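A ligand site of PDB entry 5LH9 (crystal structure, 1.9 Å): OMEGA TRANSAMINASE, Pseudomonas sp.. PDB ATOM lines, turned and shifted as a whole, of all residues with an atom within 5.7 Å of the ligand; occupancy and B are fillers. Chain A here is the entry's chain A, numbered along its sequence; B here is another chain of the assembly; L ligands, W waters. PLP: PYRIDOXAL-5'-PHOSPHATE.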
ATOM      1  N   LEU A  62     -21.643 -33.087  15.799  1.00  0.00           N
ATOM      2  CA  LEU A  62     -22.447 -32.901  17.009  1.00  0.00           C
ATOM      3  C   LEU A  62     -23.764 -33.634  16.749  1.00  0.00           C
ATOM      4  O   LEU A  62     -24.804 -33.036  16.456  1.00  0.00           O
ATOM      5  CB  LEU A  62     -22.662 -31.432  17.347  1.00  0.00           C
ATOM      6  CG  LEU A  62     -21.553 -30.745  18.160  1.00  0.00           C
ATOM      7  CD1 LEU A  62     -21.795 -29.255  18.256  1.00  0.00           C
ATOM      8  CD2 LEU A  62     -21.429 -31.361  19.550  1.00  0.00           C
ATOM      9  N   TRP A  63     -23.707 -34.968  16.862  1.00  0.00           N
ATOM     10  CA  TRP A  63     -24.820 -35.860  16.534  1.00  0.00           C
ATOM     11  C   TRP A  63     -25.497 -35.520  15.209  1.00  0.00           C
ATOM     12  O   TRP A  63     -26.707 -35.715  15.077  1.00  0.00           O
ATOM     13  CB  TRP A  63     -25.909 -35.856  17.607  1.00  0.00           C
ATOM     14  CG  TRP A  63     -25.568 -35.510  19.015  1.00  0.00           C
ATOM     15  CD1 TRP A  63     -25.160 -34.303  19.494  1.00  0.00           C
ATOM     16  CD2 TRP A  63     -25.683 -36.377  20.147  1.00  0.00           C
ATOM     17  NE1 TRP A  63     -24.992 -34.373  20.861  1.00  0.00           N
ATOM     18  CE2 TRP A  63     -25.303 -35.637  21.279  1.00  0.00           C
ATOM     19  CE3 TRP A  63     -26.068 -37.711  20.314  1.00  0.00           C
ATOM     20  CZ2 TRP A  63     -25.289 -36.179  22.565  1.00  0.00           C
ATOM     21  CZ3 TRP A  63     -26.047 -38.257  21.588  1.00  0.00           C
ATOM     22  CH2 TRP A  63     -25.665 -37.494  22.689  1.00  0.00           C
ATOM     23  N   SER A 122     -33.494 -23.124  10.561  1.00  0.00           N
ATOM     24  CA  SER A 122     -32.097 -23.400  10.278  1.00  0.00           C
ATOM     25  C   SER A 122     -31.394 -24.227  11.351  1.00  0.00           C
ATOM     26  O   SER A 122     -30.179 -24.426  11.260  1.00  0.00           O
ATOM     27  CB  SER A 122     -31.348 -22.078  10.074  1.00  0.00           C
ATOM     28  OG  SER A 122     -31.823 -21.428   8.908  1.00  0.00           O
ATOM     29  N   GLY A 123     -32.115 -24.722  12.352  1.00  0.00           N
ATOM     30  CA  GLY A 123     -31.455 -25.555  13.352  1.00  0.00           C
ATOM     31  C   GLY A 123     -32.437 -26.119  14.356  1.00  0.00           C
ATOM     32  O   GLY A 123     -33.645 -25.879  14.287  1.00  0.00           O
ATOM     33  N   GLY A 124     -31.878 -26.855  15.318  1.00  0.00           N
ATOM     34  CA  GLY A 124     -32.696 -27.502  16.326  1.00  0.00           C
ATOM     35  C   GLY A 124     -33.260 -26.505  17.326  1.00  0.00           C
ATOM     36  O   GLY A 124     -34.435 -26.586  17.704  1.00  0.00           O
ATOM     37  N   SER A 125     -32.435 -25.562  17.766  1.00  0.00           N
ATOM     38  CA  SER A 125     -32.952 -24.521  18.636  1.00  0.00           C
ATOM     39  C   SER A 125     -34.103 -23.774  17.968  1.00  0.00           C
ATOM     40  O   SER A 125     -35.120 -23.493  18.600  1.00  0.00           O
ATOM     41  CB  SER A 125     -31.826 -23.553  19.032  1.00  0.00           C
ATOM     42  OG  SER A 125     -30.800 -24.236  19.726  1.00  0.00           O
ATOM     43  N   ASP A 126     -33.961 -23.467  16.677  1.00  0.00           N
ATOM     44  CA  ASP A 126     -35.072 -22.897  15.918  1.00  0.00           C
ATOM     45  C   ASP A 126     -36.283 -23.809  15.979  1.00  0.00           C
ATOM     46  O   ASP A 126     -37.415 -23.353  16.184  1.00  0.00           O
ATOM     47  CB  ASP A 126     -34.704 -22.702  14.445  1.00  0.00           C
ATOM     48  CG  ASP A 126     -33.553 -21.769  14.240  1.00  0.00           C
ATOM     49  OD1 ASP A 126     -32.951 -21.294  15.236  1.00  0.00           O
ATOM     50  OD2 ASP A 126     -33.257 -21.512  13.054  1.00  0.00           O
ATOM     51  N   VAL A 128     -37.220 -26.088  18.055  1.00  0.00           N
ATOM     52  CA  VAL A 128     -37.852 -26.085  19.379  1.00  0.00           C
ATOM     53  C   VAL A 128     -38.595 -24.774  19.600  1.00  0.00           C
ATOM     54  O   VAL A 128     -39.793 -24.769  19.922  1.00  0.00           O
ATOM     55  CB  VAL A 128     -36.792 -26.324  20.464  1.00  0.00           C
ATOM     56  CG1 VAL A 128     -37.330 -26.016  21.860  1.00  0.00           C
ATOM     57  CG2 VAL A 128     -36.278 -27.765  20.403  1.00  0.00           C
ATOM     58  N   TYR A 157     -32.401 -31.504  26.853  1.00  0.00           N
ATOM     59  CA  TYR A 157     -31.708 -30.429  26.158  1.00  0.00           C
ATOM     60  C   TYR A 157     -32.489 -30.081  24.906  1.00  0.00           C
ATOM     61  O   TYR A 157     -32.765 -30.964  24.082  1.00  0.00           O
ATOM     62  CB  TYR A 157     -30.275 -30.814  25.794  1.00  0.00           C
ATOM     63  CG  TYR A 157     -29.570 -29.708  25.063  1.00  0.00           C
ATOM     64  CD1 TYR A 157     -29.129 -28.580  25.738  1.00  0.00           C
ATOM     65  CD2 TYR A 157     -29.347 -29.782  23.698  1.00  0.00           C
ATOM     66  CE1 TYR A 157     -28.493 -27.553  25.066  1.00  0.00           C
ATOM     67  CE2 TYR A 157     -28.704 -28.768  23.018  1.00  0.00           C
ATOM     68  CZ  TYR A 157     -28.278 -27.655  23.714  1.00  0.00           C
ATOM     69  OH  TYR A 157     -27.644 -26.641  23.037  1.00  0.00           O
ATOM     70  N   HIS A 158     -32.808 -28.796  24.757  1.00  0.00           N
ATOM     71  CA  HIS A 158     -33.715 -28.355  23.708  1.00  0.00           C
ATOM     72  C   HIS A 158     -33.217 -27.084  23.033  1.00  0.00           C
ATOM     73  O   HIS A 158     -34.026 -26.243  22.605  1.00  0.00           O
ATOM     74  CB  HIS A 158     -35.112 -28.146  24.291  1.00  0.00           C
ATOM     75  CG  HIS A 158     -35.672 -29.359  24.963  1.00  0.00           C
ATOM     76  ND1 HIS A 158     -35.990 -30.513  24.282  1.00  0.00           N
ATOM     77  CD2 HIS A 158     -35.966 -29.598  26.263  1.00  0.00           C
ATOM     78  CE1 HIS A 158     -36.456 -31.414  25.134  1.00  0.00           C
ATOM     79  NE2 HIS A 158     -36.447 -30.882  26.341  1.00  0.00           N
ATOM     80  N   GLY A 159     -31.912 -26.926  22.919  1.00  0.00           N
ATOM     81  CA  GLY A 159     -31.344 -25.754  22.281  1.00  0.00           C
ATOM     82  C   GLY A 159     -31.096 -24.626  23.268  1.00  0.00           C
ATOM     83  O   GLY A 159     -31.233 -24.767  24.486  1.00  0.00           O
ATOM     84  N   VAL A 160     -30.732 -23.468  22.718  1.00  0.00           N
ATOM     85  CA  VAL A 160     -30.214 -22.374  23.526  1.00  0.00           C
ATOM     86  C   VAL A 160     -30.883 -21.045  23.200  1.00  0.00           C
ATOM     87  O   VAL A 160     -30.444 -19.991  23.660  1.00  0.00           O
ATOM     88  CB  VAL A 160     -28.690 -22.245  23.380  1.00  0.00           C
ATOM     89  CG1 VAL A 160     -28.009 -23.468  23.951  1.00  0.00           C
ATOM     90  CG2 VAL A 160     -28.311 -22.070  21.911  1.00  0.00           C
ATOM     91  N   GLU A 231     -37.295 -35.597  24.612  1.00  0.00           N
ATOM     92  CA  GLU A 231     -36.496 -36.328  23.634  1.00  0.00           C
ATOM     93  C   GLU A 231     -36.796 -37.820  23.755  1.00  0.00           C
ATOM     94  O   GLU A 231     -36.761 -38.370  24.861  1.00  0.00           O
ATOM     95  CB  GLU A 231     -35.016 -36.091  23.870  1.00  0.00           C
ATOM     96  CG  GLU A 231     -34.608 -34.645  23.843  1.00  0.00           C
ATOM     97  CD  GLU A 231     -33.367 -34.392  24.664  1.00  0.00           C
ATOM     98  OE1 GLU A 231     -32.256 -34.651  24.140  1.00  0.00           O
ATOM     99  OE2 GLU A 231     -33.508 -33.958  25.830  1.00  0.00           O
ATOM    100  N   GLY A 235     -30.212 -36.836  24.687  1.00  0.00           N
ATOM    101  CA  GLY A 235     -28.861 -36.865  24.174  1.00  0.00           C
ATOM    102  C   GLY A 235     -27.843 -36.186  25.072  1.00  0.00           C
ATOM    103  O   GLY A 235     -27.147 -36.851  25.845  1.00  0.00           O
ATOM    104  N   ALA A 236     -27.758 -34.855  24.984  1.00  0.00           N
ATOM    105  CA  ALA A 236     -26.742 -34.116  25.718  1.00  0.00           C
ATOM    106  C   ALA A 236     -26.851 -34.315  27.225  1.00  0.00           C
ATOM    107  O   ALA A 236     -25.859 -34.123  27.942  1.00  0.00           O
ATOM    108  CB  ALA A 236     -26.827 -32.627  25.380  1.00  0.00           C
ATOM    109  N   ASP A 264     -38.931 -33.756  20.678  1.00  0.00           N
ATOM    110  CA  ASP A 264     -37.677 -33.167  20.223  1.00  0.00           C
ATOM    111  C   ASP A 264     -36.866 -34.278  19.556  1.00  0.00           C
ATOM    112  O   ASP A 264     -36.085 -34.974  20.194  1.00  0.00           O
ATOM    113  CB  ASP A 264     -36.929 -32.531  21.383  1.00  0.00           C
ATOM    114  CG  ASP A 264     -35.665 -31.809  20.944  1.00  0.00           C
ATOM    115  OD1 ASP A 264     -35.170 -32.107  19.834  1.00  0.00           O
ATOM    116  OD2 ASP A 264     -35.166 -30.962  21.715  1.00  0.00           O
ATOM    117  N   VAL A 266     -34.535 -33.826  17.274  1.00  0.00           N
ATOM    118  CA  VAL A 266     -33.378 -33.216  16.621  1.00  0.00           C
ATOM    119  C   VAL A 266     -32.240 -34.233  16.507  1.00  0.00           C
ATOM    120  O   VAL A 266     -31.530 -34.282  15.496  1.00  0.00           O
ATOM    121  CB  VAL A 266     -32.949 -31.953  17.383  1.00  0.00           C
ATOM    122  CG1 VAL A 266     -31.542 -31.510  16.970  1.00  0.00           C
ATOM    123  CG2 VAL A 266     -33.957 -30.840  17.137  1.00  0.00           C
ATOM    124  N   VAL A 267     -32.059 -35.064  17.538  1.00  0.00           N
ATOM    125  CA  VAL A 267     -31.015 -36.083  17.497  1.00  0.00           C
ATOM    126  C   VAL A 267     -31.543 -37.399  16.938  1.00  0.00           C
ATOM    127  O   VAL A 267     -30.943 -38.006  16.051  1.00  0.00           O
ATOM    128  CB  VAL A 267     -30.413 -36.283  18.903  1.00  0.00           C
ATOM    129  CG1 VAL A 267     -29.490 -37.496  18.935  1.00  0.00           C
ATOM    130  CG2 VAL A 267     -29.647 -35.044  19.320  1.00  0.00           C
ATOM    131  N   ALA A 292     -33.724 -31.454  13.027  1.00  0.00           N
ATOM    132  CA  ALA A 292     -32.557 -30.700  12.572  1.00  0.00           C
ATOM    133  C   ALA A 292     -31.398 -31.687  12.419  1.00  0.00           C
ATOM    134  O   ALA A 292     -31.611 -32.837  12.070  1.00  0.00           O
ATOM    135  CB  ALA A 292     -32.210 -29.582  13.544  1.00  0.00           C
ATOM    136  N   LYS A 293     -30.190 -31.211  12.693  1.00  0.00           N
ATOM    137  CA  LYS A 293     -28.969 -32.045  12.665  1.00  0.00           C
ATOM    138  C   LYS A 293     -28.984 -32.981  11.485  1.00  0.00           C
ATOM    139  O   LYS A 293     -28.616 -32.582  10.391  1.00  0.00           O
ATOM    140  CB  LYS A 293     -28.831 -32.784  13.974  1.00  0.00           C
ATOM    141  CG  LYS A 293     -28.460 -31.777  15.078  1.00  0.00           C
ATOM    142  CD  LYS A 293     -28.070 -32.447  16.420  1.00  0.00           C
ATOM    143  CE  LYS A 293     -27.616 -31.378  17.444  1.00  0.00           C
ATOM    144  NZ  LYS A 293     -28.348 -31.522  18.729  1.00  0.00           N
ATOM    145  N   PHE B  91     -17.453 -26.385  19.227  1.00  0.00           N
ATOM    146  CA  PHE B  91     -17.656 -26.389  20.669  1.00  0.00           C
ATOM    147  C   PHE B  91     -16.323 -26.587  21.393  1.00  0.00           C
ATOM    148  O   PHE B  91     -15.310 -26.962  20.797  1.00  0.00           O
ATOM    149  CB  PHE B  91     -18.667 -27.474  21.054  1.00  0.00           C
ATOM    150  CG  PHE B  91     -20.105 -27.128  20.749  1.00  0.00           C
ATOM    151  CD1 PHE B  91     -20.424 -26.235  19.736  1.00  0.00           C
ATOM    152  CD2 PHE B  91     -21.126 -27.706  21.472  1.00  0.00           C
ATOM    153  CE1 PHE B  91     -21.739 -25.924  19.463  1.00  0.00           C
ATOM    154  CE2 PHE B  91     -22.451 -27.394  21.201  1.00  0.00           C
ATOM    155  CZ  PHE B  91     -22.758 -26.498  20.195  1.00  0.00           C
ATOM    156  N   GLY B 328     -24.648 -21.630  22.374  1.00  0.00           N
ATOM    157  CA  GLY B 328     -24.177 -21.752  21.008  1.00  0.00           C
ATOM    158  C   GLY B 328     -24.930 -22.840  20.290  1.00  0.00           C
ATOM    159  O   GLY B 328     -25.707 -23.599  20.873  1.00  0.00           O
ATOM    160  N   TYR B 329     -24.645 -22.937  19.003  1.00  0.00           N
ATOM    161  CA  TYR B 329     -25.445 -23.727  18.080  1.00  0.00           C
ATOM    162  C   TYR B 329     -24.583 -24.746  17.364  1.00  0.00           C
ATOM    163  O   TYR B 329     -23.403 -24.511  17.094  1.00  0.00           O
ATOM    164  CB  TYR B 329     -26.144 -22.800  17.080  1.00  0.00           C
ATOM    165  CG  TYR B 329     -26.929 -21.712  17.770  1.00  0.00           C
ATOM    166  CD1 TYR B 329     -28.181 -21.967  18.301  1.00  0.00           C
ATOM    167  CD2 TYR B 329     -26.389 -20.446  17.935  1.00  0.00           C
ATOM    168  CE1 TYR B 329     -28.887 -20.983  18.950  1.00  0.00           C
ATOM    169  CE2 TYR B 329     -27.096 -19.452  18.581  1.00  0.00           C
ATOM    170  CZ  TYR B 329     -28.343 -19.724  19.095  1.00  0.00           C
ATOM    171  OH  TYR B 329     -29.039 -18.740  19.741  1.00  0.00           O
ATOM    172  N   THR B 330     -25.175 -25.899  17.074  1.00  0.00           N
ATOM    173  CA  THR B 330     -24.488 -26.920  16.290  1.00  0.00           C
ATOM    174  C   THR B 330     -23.801 -26.308  15.080  1.00  0.00           C
ATOM    175  O   THR B 330     -22.632 -26.586  14.800  1.00  0.00           O
ATOM    176  CB  THR B 330     -25.490 -27.997  15.863  1.00  0.00           C
ATOM    177  OG1 THR B 330     -26.037 -28.640  17.020  1.00  0.00           O
ATOM    178  CG2 THR B 330     -24.827 -29.039  14.961  1.00  0.00           C
ATOM    179  N   TYR B 331     -24.502 -25.420  14.371  1.00  0.00           N
ATOM    180  CA  TYR B 331     -23.990 -24.838  13.135  1.00  0.00           C
ATOM    181  C   TYR B 331     -23.273 -23.506  13.367  1.00  0.00           C
ATOM    182  O   TYR B 331     -22.951 -22.811  12.402  1.00  0.00           O
ATOM    183  CB  TYR B 331     -25.125 -24.683  12.125  1.00  0.00           C
ATOM    184  CG  TYR B 331     -25.707 -26.017  11.710  1.00  0.00           C
ATOM    185  CD1 TYR B 331     -24.861 -27.065  11.341  1.00  0.00           C
ATOM    186  CD2 TYR B 331     -27.082 -26.255  11.697  1.00  0.00           C
ATOM    187  CE1 TYR B 331     -25.360 -28.289  10.983  1.00  0.00           C
ATOM    188  CE2 TYR B 331     -27.594 -27.482  11.332  1.00  0.00           C
ATOM    189  CZ  TYR B 331     -26.724 -28.506  10.970  1.00  0.00           C
ATOM    190  OH  TYR B 331     -27.206 -29.743  10.600  1.00  0.00           O
HETATM  191  N1  PLP L   1     -32.658 -30.291  20.903  1.00  0.00           N
HETATM  192  C2  PLP L   1     -31.893 -31.391  20.985  1.00  0.00           C
HETATM  193  C2A PLP L   1     -32.459 -32.707  21.574  1.00  0.00           C
HETATM  194  C3  PLP L   1     -30.552 -31.355  20.540  1.00  0.00           C
HETATM  195  O3  PLP L   1     -29.765 -32.512  20.636  1.00  0.00           O
HETATM  196  C4  PLP L   1     -29.997 -30.222  20.008  1.00  0.00           C
HETATM  197  C4A PLP L   1     -28.468 -30.309  19.508  1.00  0.00           C
HETATM  198  C5  PLP L   1     -30.776 -29.096  19.910  1.00  0.00           C
HETATM  199  C6  PLP L   1     -32.102 -29.117  20.367  1.00  0.00           C
HETATM  200  C5A PLP L   1     -30.212 -27.752  19.344  1.00  0.00           C
HETATM  201  O4P PLP L   1     -29.810 -27.862  17.994  1.00  0.00           O
HETATM  202  P   PLP L   1     -28.916 -26.746  17.412  1.00  0.00           P
HETATM  203  O1P PLP L   1     -29.504 -25.353  17.657  1.00  0.00           O
HETATM  204  O2P PLP L   1     -27.599 -26.831  18.067  1.00  0.00           O
HETATM  205  O3P PLP L   1     -28.771 -26.978  15.940  1.00  0.00           O
HETATM  206  O   HOH W   1     -28.720 -28.766  13.933  1.00  0.00           O
HETATM  207  O   HOH W   2     -27.394 -25.132  14.774  1.00  0.00           O
HETATM  208  O   HOH W   3     -32.195 -36.111  21.977  1.00  0.00           O
HETATM  209  O   HOH W   4     -29.659 -33.609  23.376  1.00  0.00           O
HETATM  210  O   HOH W   5     -31.029 -23.503  15.796  1.00  0.00           O
HETATM  211  O   HOH W   6     -27.139 -25.955  20.595  1.00  0.00           O
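Water W2 lies within hydrogen-bond range of O3P of the ligand, N of Tyr 331 of chain B and N of Thr 330 of chain B.
Water W1 lies within hydrogen-bond range of an oxygen (O3P) of the ligand (2.7 Å) and the backbone NH (N) of Lys 293 (3.1 Å).
Water W6 lies within hydrogen-bond range of OH of Tyr 157 (2.6 Å), O2P of the ligand (2.7 Å) and O of Gly 328 of chain B (2.8 Å).
Water W4 lies within hydrogen-bond range of N of Ala 236, OE1 of Glu 231 and O3 of the ligand.
Water W5 lies within hydrogen-bond range of the side-chain carboxylate (OD1) of Asp 126 (3.0 Å), an oxygen (O1P) of the ligand (3.0 Å), the backbone NH (N) of Ser 125 (3.2 Å) and the backbone NH (N) of Gly 124 (3.5 Å).
Water W3 bridges the side-chain carboxylate (OE1) of Glu 231 and the backbone NH (N) of Gly 235.
The side-chain amino group (NZ) of Lys 293 is covalently linked to a carbon (C4A) of the ligand, at 1.4 Å.
An oxygen (O2P) of the ligand sits at hydrogen-bond distance from the backbone NH of Thr 330 of chain B (2.8 Å).
O2P of the ligand lies within hydrogen-bond range of OG1 of Thr 330 of chain B (2.6 Å).
The backbone NH of Ser 125 is in hydrogen-bond range of an oxygen (O1P) of the ligand, 2.9 Å away.
The side-chain hydroxyl (OG) of Ser 125 is in hydrogen-bond range of an oxygen (O1P) of the ligand (2.7 Å).
OD2 of Asp 264 sits at hydrogen-bond distance from N1 of the ligand, at 2.7 Å.
N of Gly 124 lies within hydrogen-bond range of O3P of the ligand, 3.2 Å away.
O of Tyr 157 sits close to N1 of the ligand (3.3 Å).
Gly 123 touches the ligand (CA to O3P, 3.99 Å).
C of His 158 touches C6 of the ligand, at 3.5 Å.
Gly 159 touches the ligand (N to C6, 3.4 Å).
OE1 of Glu 231 touches C2A of the ligand (3.2 Å).
Val 266 touches the ligand.
Val 267 touches the ligand.
CD1 of Tyr 329 of chain B touches O1P of the ligand, at 3.7 Å.
Hydrophobic or aromatic side chains that line the ligand: Tyr 157, Val 266, Val 267 and Tyr 329 of chain B.
13 residues have an atom within 4 Å of the ligand: Gly 123, Gly 124, Ser 125, Tyr 157, His 158, Gly 159, Glu 231, Asp 264, Val 266, Val 267, Lys 293, Tyr 329 of chain B and Thr 330 of chain B.
The nearest printed residue that does not touch the ligand is Val 128 (4.4 Å).
The backbone carbonyl oxygen (O) of Lys 293 sits at hydrogen-bond distance from the side-chain hydroxyl (OH) of Tyr 331 of chain B.
The side-chain hydroxyl (OG) of Ser 125 is in hydrogen-bond range of the backbone NH (N) of Val 160, at 3.1 Å.
The side-chain carboxylate (OD2) of Asp 264 is in hydrogen-bond range of a ring nitrogen (ND1) of His 158, 2.7 Å away.
The side-chain carboxylate (OD1) of Asp 264 sits at hydrogen-bond distance from the backbone NH (N) of Val 266.
The backbone NH (N) of Tyr 157 is in hydrogen-bond range of the side-chain carboxylate (OE2) of Glu 231, at 2.9 Å.
OE1 of Glu 231 lies within hydrogen-bond range of N of Gly 235, 3.0 Å away.
The backbone NH of Gly 123 lies within hydrogen-bond range of the side-chain carboxylate of Asp 126.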
